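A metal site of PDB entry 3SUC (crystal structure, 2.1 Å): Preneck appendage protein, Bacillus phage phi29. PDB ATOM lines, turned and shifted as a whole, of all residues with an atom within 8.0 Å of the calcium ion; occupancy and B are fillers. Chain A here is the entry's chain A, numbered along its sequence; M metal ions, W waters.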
ATOM      1  N   LEU A 157      16.729   6.609   3.835  1.00  0.00           N
ATOM      2  CA  LEU A 157      17.358   6.332   5.113  1.00  0.00           C
ATOM      3  C   LEU A 157      17.618   7.667   5.825  1.00  0.00           C
ATOM      4  O   LEU A 157      16.704   8.262   6.394  1.00  0.00           O
ATOM      5  CB  LEU A 157      18.677   5.579   4.916  1.00  0.00           C
ATOM      6  CG  LEU A 157      19.106   4.408   5.819  1.00  0.00           C
ATOM      7  CD1 LEU A 157      20.619   4.400   5.968  1.00  0.00           C
ATOM      8  CD2 LEU A 157      18.459   4.434   7.200  1.00  0.00           C
ATOM      9  N   HIS A 158      18.865   8.123   5.774  1.00  0.00           N
ATOM     10  CA  HIS A 158      19.265   9.380   6.399  1.00  0.00           C
ATOM     11  C   HIS A 158      19.314  10.518   5.390  1.00  0.00           C
ATOM     12  O   HIS A 158      19.372  10.284   4.184  1.00  0.00           O
ATOM     13  CB  HIS A 158      20.633   9.245   7.074  1.00  0.00           C
ATOM     14  CG  HIS A 158      20.739   8.080   8.012  1.00  0.00           C
ATOM     15  ND1 HIS A 158      19.898   7.902   9.092  1.00  0.00           N
ATOM     16  CD2 HIS A 158      21.606   7.036   8.032  1.00  0.00           C
ATOM     17  CE1 HIS A 158      20.239   6.795   9.730  1.00  0.00           C
ATOM     18  NE2 HIS A 158      21.272   6.248   9.109  1.00  0.00           N
ATOM     19  N   PHE A 195      12.817  12.113   6.254  1.00  0.00           N
ATOM     20  CA  PHE A 195      13.780  11.015   6.209  1.00  0.00           C
ATOM     21  C   PHE A 195      13.212   9.743   6.839  1.00  0.00           C
ATOM     22  O   PHE A 195      12.202   9.797   7.541  1.00  0.00           O
ATOM     23  CB  PHE A 195      15.099  11.419   6.899  1.00  0.00           C
ATOM     24  CG  PHE A 195      14.913  12.155   8.205  1.00  0.00           C
ATOM     25  CD1 PHE A 195      14.827  13.550   8.232  1.00  0.00           C
ATOM     26  CD2 PHE A 195      14.829  11.446   9.406  1.00  0.00           C
ATOM     27  CE1 PHE A 195      14.649  14.227   9.440  1.00  0.00           C
ATOM     28  CE2 PHE A 195      14.652  12.114  10.613  1.00  0.00           C
ATOM     29  CZ  PHE A 195      14.567  13.510  10.630  1.00  0.00           C
ATOM     30  N   GLY A 196      13.864   8.622   6.574  1.00  0.00           N
ATOM     31  CA  GLY A 196      13.404   7.319   7.040  1.00  0.00           C
ATOM     32  C   GLY A 196      13.864   6.971   8.438  1.00  0.00           C
ATOM     33  O   GLY A 196      13.104   6.439   9.244  1.00  0.00           O
ATOM     34  N   ASP A 197      15.136   7.260   8.709  1.00  0.00           N
ATOM     35  CA  ASP A 197      15.709   7.034  10.023  1.00  0.00           C
ATOM     36  C   ASP A 197      16.041   8.360  10.695  1.00  0.00           C
ATOM     37  O   ASP A 197      15.206   8.913  11.422  1.00  0.00           O
ATOM     38  CB  ASP A 197      16.958   6.143   9.908  1.00  0.00           C
ATOM     39  CG  ASP A 197      17.310   5.461  11.222  1.00  0.00           C
ATOM     40  OD1 ASP A 197      18.338   4.745  11.246  1.00  0.00           O
ATOM     41  OD2 ASP A 197      16.581   5.636  12.227  1.00  0.00           O
ATOM     42  N   ASP A 198      17.238   8.888  10.430  1.00  0.00           N
ATOM     43  CA  ASP A 198      17.722  10.084  11.120  1.00  0.00           C
ATOM     44  C   ASP A 198      18.145  11.182  10.144  1.00  0.00           C
ATOM     45  O   ASP A 198      18.725  10.896   9.103  1.00  0.00           O
ATOM     46  CB  ASP A 198      18.892   9.719  12.035  1.00  0.00           C
ATOM     47  CG  ASP A 198      18.536   8.645  13.036  1.00  0.00           C
ATOM     48  OD1 ASP A 198      17.563   8.817  13.794  1.00  0.00           O
ATOM     49  OD2 ASP A 198      19.241   7.605  13.064  1.00  0.00           O
ATOM     50  N   GLY A 199      17.832  12.425  10.501  1.00  0.00           N
ATOM     51  CA  GLY A 199      18.165  13.586   9.682  1.00  0.00           C
ATOM     52  C   GLY A 199      19.647  13.729   9.396  1.00  0.00           C
ATOM     53  O   GLY A 199      20.085  13.604   8.251  1.00  0.00           O
ATOM     54  N   THR A 201      23.399  12.239  10.990  1.00  0.00           N
ATOM     55  CA  THR A 201      23.889  11.176  11.878  1.00  0.00           C
ATOM     56  C   THR A 201      25.357  10.795  11.648  1.00  0.00           C
ATOM     57  O   THR A 201      25.874  10.897  10.532  1.00  0.00           O
ATOM     58  CB  THR A 201      23.001   9.910  11.796  1.00  0.00           C
ATOM     59  OG1 THR A 201      23.551   8.871  12.617  1.00  0.00           O
ATOM     60  CG2 THR A 201      22.889   9.403  10.372  1.00  0.00           C
ATOM     61  N   HIS A 203      28.436   7.691  12.680  1.00  0.00           N
ATOM     62  CA  HIS A 203      28.753   6.347  13.166  1.00  0.00           C
ATOM     63  C   HIS A 203      30.252   6.123  13.088  1.00  0.00           C
ATOM     64  O   HIS A 203      30.903   6.579  12.159  1.00  0.00           O
ATOM     65  CB  HIS A 203      28.062   5.270  12.336  1.00  0.00           C
ATOM     66  CG  HIS A 203      26.575   5.402  12.273  1.00  0.00           C
ATOM     67  ND1 HIS A 203      25.933   6.164  11.326  1.00  0.00           N
ATOM     68  CD2 HIS A 203      25.597   4.845  13.032  1.00  0.00           C
ATOM     69  CE1 HIS A 203      24.628   6.091  11.503  1.00  0.00           C
ATOM     70  NE2 HIS A 203      24.398   5.289  12.529  1.00  0.00           N
ATOM     71  N   ALA A 222       9.666   5.163  14.070  1.00  0.00           N
ATOM     72  CA  ALA A 222      10.653   4.424  14.845  1.00  0.00           C
ATOM     73  C   ALA A 222      11.641   5.385  15.526  1.00  0.00           C
ATOM     74  O   ALA A 222      11.248   6.479  15.964  1.00  0.00           O
ATOM     75  CB  ALA A 222      11.394   3.405  13.969  1.00  0.00           C
ATOM     76  N   ASN A 223      12.911   4.977  15.612  1.00  0.00           N
ATOM     77  CA  ASN A 223      13.941   5.831  16.210  1.00  0.00           C
ATOM     78  C   ASN A 223      14.332   6.946  15.235  1.00  0.00           C
ATOM     79  O   ASN A 223      15.441   6.973  14.696  1.00  0.00           O
ATOM     80  CB  ASN A 223      15.148   4.991  16.645  1.00  0.00           C
ATOM     81  CG  ASN A 223      15.920   5.623  17.795  1.00  0.00           C
ATOM     82  OD1 ASN A 223      15.337   6.207  18.711  1.00  0.00           O
ATOM     83  ND2 ASN A 223      17.247   5.510  17.747  1.00  0.00           N
ATOM     84  N   CYS A 224      13.401   7.874  15.038  1.00  0.00           N
ATOM     85  CA  CYS A 224      13.546   8.944  14.073  1.00  0.00           C
ATOM     86  C   CYS A 224      14.003  10.222  14.742  1.00  0.00           C
ATOM     87  O   CYS A 224      13.203  11.046  15.170  1.00  0.00           O
ATOM     88  CB  CYS A 224      12.222   9.173  13.330  1.00  0.00           C
ATOM     89  SG  CYS A 224      11.713   7.817  12.267  1.00  0.00           S
ATOM     90  N   ASN A 225      15.324  10.368  14.806  1.00  0.00           N
ATOM     91  CA  ASN A 225      15.937  11.460  15.536  1.00  0.00           C
ATOM     92  C   ASN A 225      16.439  12.559  14.611  1.00  0.00           C
ATOM     93  O   ASN A 225      17.020  12.263  13.569  1.00  0.00           O
ATOM     94  CB  ASN A 225      17.083  10.926  16.410  1.00  0.00           C
ATOM     95  CG  ASN A 225      16.628   9.845  17.387  1.00  0.00           C
ATOM     96  OD1 ASN A 225      15.637  10.010  18.103  1.00  0.00           O
ATOM     97  ND2 ASN A 225      17.359   8.746  17.418  1.00  0.00           N
ATOM     98  N   GLY A 226      16.195  13.804  15.001  1.00  0.00           N
ATOM     99  CA  GLY A 226      16.726  14.963  14.276  1.00  0.00           C
ATOM    100  C   GLY A 226      18.228  14.853  14.080  1.00  0.00           C
ATOM    101  O   GLY A 226      18.725  14.844  12.950  1.00  0.00           O
ATOM    102  N   PHE A 227      18.956  14.759  15.181  1.00  0.00           N
ATOM    103  CA  PHE A 227      20.388  14.493  15.137  1.00  0.00           C
ATOM    104  C   PHE A 227      20.645  13.244  15.966  1.00  0.00           C
ATOM    105  O   PHE A 227      20.139  13.133  17.082  1.00  0.00           O
ATOM    106  CB  PHE A 227      21.179  15.674  15.689  1.00  0.00           C
ATOM    107  CG  PHE A 227      20.998  16.945  14.904  1.00  0.00           C
ATOM    108  CD1 PHE A 227      19.885  17.758  15.102  1.00  0.00           C
ATOM    109  CD2 PHE A 227      21.955  17.348  13.984  1.00  0.00           C
ATOM    110  CE1 PHE A 227      19.712  18.921  14.384  1.00  0.00           C
ATOM    111  CE2 PHE A 227      21.801  18.523  13.258  1.00  0.00           C
ATOM    112  CZ  PHE A 227      20.679  19.315  13.454  1.00  0.00           C
ATOM    113  N   GLU A 228      21.390  12.299  15.402  1.00  0.00           N
ATOM    114  CA  GLU A 228      21.738  11.090  16.138  1.00  0.00           C
ATOM    115  C   GLU A 228      23.225  10.773  16.058  1.00  0.00           C
ATOM    116  O   GLU A 228      23.724  10.379  15.012  1.00  0.00           O
ATOM    117  CB  GLU A 228      20.904   9.892  15.693  1.00  0.00           C
ATOM    118  CG  GLU A 228      21.215   8.623  16.481  1.00  0.00           C
ATOM    119  CD  GLU A 228      20.392   7.423  16.057  1.00  0.00           C
ATOM    120  OE1 GLU A 228      20.998   6.358  15.797  1.00  0.00           O
ATOM    121  OE2 GLU A 228      19.148   7.537  15.996  1.00  0.00           O
ATOM    122  N   ASP A 230      25.488   8.227  16.869  1.00  0.00           N
ATOM    123  CA  ASP A 230      25.275   6.806  17.165  1.00  0.00           C
ATOM    124  C   ASP A 230      26.561   5.980  17.291  1.00  0.00           C
ATOM    125  O   ASP A 230      27.653   6.533  17.410  1.00  0.00           O
ATOM    126  CB  ASP A 230      24.338   6.187  16.114  1.00  0.00           C
ATOM    127  CG  ASP A 230      23.633   4.930  16.601  1.00  0.00           C
ATOM    128  OD1 ASP A 230      23.629   4.660  17.828  1.00  0.00           O
ATOM    129  OD2 ASP A 230      23.072   4.189  15.764  1.00  0.00           O
ATOM    130  N   TYR A 247      11.594  12.299  17.125  1.00  0.00           N
ATOM    131  CA  TYR A 247      11.575  11.627  18.413  1.00  0.00           C
ATOM    132  C   TYR A 247      12.602  12.288  19.350  1.00  0.00           C
ATOM    133  O   TYR A 247      12.227  13.023  20.259  1.00  0.00           O
ATOM    134  CB  TYR A 247      11.815  10.116  18.294  1.00  0.00           C
ATOM    135  CG  TYR A 247      12.046   9.440  19.636  1.00  0.00           C
ATOM    136  CD1 TYR A 247      11.109   9.562  20.671  1.00  0.00           C
ATOM    137  CD2 TYR A 247      13.209   8.710  19.882  1.00  0.00           C
ATOM    138  CE1 TYR A 247      11.326   8.968  21.902  1.00  0.00           C
ATOM    139  CE2 TYR A 247      13.436   8.107  21.113  1.00  0.00           C
ATOM    140  CZ  TYR A 247      12.489   8.241  22.128  1.00  0.00           C
ATOM    141  OH  TYR A 247      12.696   7.648  23.350  1.00  0.00           O
ATOM    142  N   GLU A 251      20.110  12.721  19.902  1.00  0.00           N
ATOM    143  CA  GLU A 251      20.353  11.467  20.590  1.00  0.00           C
ATOM    144  C   GLU A 251      21.834  11.099  20.514  1.00  0.00           C
ATOM    145  O   GLU A 251      22.423  11.060  19.442  1.00  0.00           O
ATOM    146  CB  GLU A 251      19.486  10.340  20.033  1.00  0.00           C
ATOM    147  CG  GLU A 251      19.738   8.988  20.709  1.00  0.00           C
ATOM    148  CD  GLU A 251      18.720   7.928  20.318  1.00  0.00           C
ATOM    149  OE1 GLU A 251      18.822   7.395  19.196  1.00  0.00           O
ATOM    150  OE2 GLU A 251      17.827   7.635  21.131  1.00  0.00           O
ATOM    151  N   LYS A 253      23.767   7.906  21.562  1.00  0.00           N
ATOM    152  CA  LYS A 253      23.553   6.542  22.056  1.00  0.00           C
ATOM    153  C   LYS A 253      24.450   5.503  21.383  1.00  0.00           C
ATOM    154  O   LYS A 253      25.454   5.834  20.758  1.00  0.00           O
ATOM    155  CB  LYS A 253      22.074   6.157  21.920  1.00  0.00           C
ATOM    156  CG  LYS A 253      21.635   5.832  20.501  1.00  0.00           C
ATOM    157  CD  LYS A 253      20.477   4.852  20.510  1.00  0.00           C
ATOM    158  CE  LYS A 253      20.395   4.081  19.205  1.00  0.00           C
ATOM    159  NZ  LYS A 253      20.251   4.968  18.031  1.00  0.00           N
ATOM    160  N   HIS A 255      23.907   0.883  20.183  1.00  0.00           N
ATOM    161  CA  HIS A 255      23.150  -0.357  20.319  1.00  0.00           C
ATOM    162  C   HIS A 255      23.921  -1.316  21.235  1.00  0.00           C
ATOM    163  O   HIS A 255      25.096  -1.082  21.548  1.00  0.00           O
ATOM    164  CB  HIS A 255      22.899  -1.005  18.946  1.00  0.00           C
ATOM    165  CG  HIS A 255      22.184  -0.095  17.975  1.00  0.00           C
ATOM    166  ND1 HIS A 255      20.917   0.396  18.211  1.00  0.00           N
ATOM    167  CD2 HIS A 255      22.549   0.388  16.771  1.00  0.00           C
ATOM    168  CE1 HIS A 255      20.539   1.150  17.198  1.00  0.00           C
ATOM    169  NE2 HIS A 255      21.518   1.166  16.312  1.00  0.00           N
ATOM    170  N   ARG A 281      21.753   7.539  26.073  1.00  0.00           N
ATOM    171  CA  ARG A 281      21.579   6.179  26.568  1.00  0.00           C
ATOM    172  C   ARG A 281      22.560   5.206  25.914  1.00  0.00           C
ATOM    173  O   ARG A 281      23.240   5.566  24.964  1.00  0.00           O
ATOM    174  CB  ARG A 281      20.142   5.709  26.332  1.00  0.00           C
ATOM    175  CG  ARG A 281      19.707   5.792  24.882  1.00  0.00           C
ATOM    176  CD  ARG A 281      18.227   6.094  24.749  1.00  0.00           C
ATOM    177  NE  ARG A 281      17.793   6.030  23.352  1.00  0.00           N
ATOM    178  CZ  ARG A 281      17.233   4.963  22.788  1.00  0.00           C
ATOM    179  NH1 ARG A 281      17.031   3.849  23.484  1.00  0.00           N
ATOM    180  NH2 ARG A 281      16.887   5.004  21.507  1.00  0.00           N
ATOM    181  N   GLN A 316       8.199   5.533  18.933  1.00  0.00           N
ATOM    182  CA  GLN A 316       8.740   4.549  19.881  1.00  0.00           C
ATOM    183  C   GLN A 316       7.683   3.935  20.803  1.00  0.00           C
ATOM    184  O   GLN A 316       7.872   3.876  22.029  1.00  0.00           O
ATOM    185  CB  GLN A 316       9.864   5.181  20.716  1.00  0.00           C
ATOM    186  CG  GLN A 316      11.058   5.681  19.924  1.00  0.00           C
ATOM    187  CD  GLN A 316      12.169   4.657  19.800  1.00  0.00           C
ATOM    188  OE1 GLN A 316      12.530   4.258  18.690  1.00  0.00           O
ATOM    189  NE2 GLN A 316      12.715   4.229  20.927  1.00  0.00           N
HETATM  190 CA    CA M   1      17.501   6.137  14.503  1.00  0.00          CA
HETATM  191 MG    MG M   2      21.968   4.885  13.661  1.00  0.00          MG
HETATM  192  O   HOH W   1      19.520   4.784  13.863  1.00  0.00           O
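The side-chain amino group (NZ) of Lys 253 sits close to the side-chain amide nitrogen (ND2) of Asn 223 (3.1 Å). ND2 of Asn 225 lies close to ND2 of Asn 223. OD1 of Asp 198 sits close to N of Asn 225. The side-chain amino group (NZ) of Lys 253 is in salt-bridge range of the side-chain carboxylate (OE1) of Glu 228 (2.7 Å). The side-chain sulfur (SG) of Cys 224 sits close to the backbone carbonyl oxygen (O) of Asp 197, 3.8 Å away. N of Asp 198 lies within hydrogen-bond range of ND1 of His 158, at 3.1 Å. The side-chain amide oxygen (OD1) of Asn 223 is in hydrogen-bond range of the guanidinium group (NH2) of Arg 281, at 3.4 Å. O of Asn 225 sits at hydrogen-bond distance from N of Gly 199 (3.2 Å).
Asn 225 touches the calcium ion (ND2 to CA, 3.9 Å). Within 4 Å of the calcium ion: Asp 197, Asp 198, Asn 223, Asn 225 and Glu 228. The nearest printed residue that does not touch the calcium ion is Cys 224 (4.5 Å).
O of Asn 223 binds the calcium ion, 2.2 Å away. OD2 of Asp 197 is bound to the calcium ion, at 2.5 Å. The calcium ion is bound by water W1 (2.5 Å). OE2 of Glu 228 binds the calcium ion, 2.6 Å away. OD2 of Asp 198 binds the calcium ion (2.7 Å). The calcium ion is bound by OD1 of Asp 198. The calcium ion has six donor atoms within binding distance.
Water W1 lies within hydrogen-bond range of the side-chain carboxylate (OD1) of Asp 197 (2.9 Å) and the side-chain carboxylate (OE1) of Glu 228 (2.9 Å).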
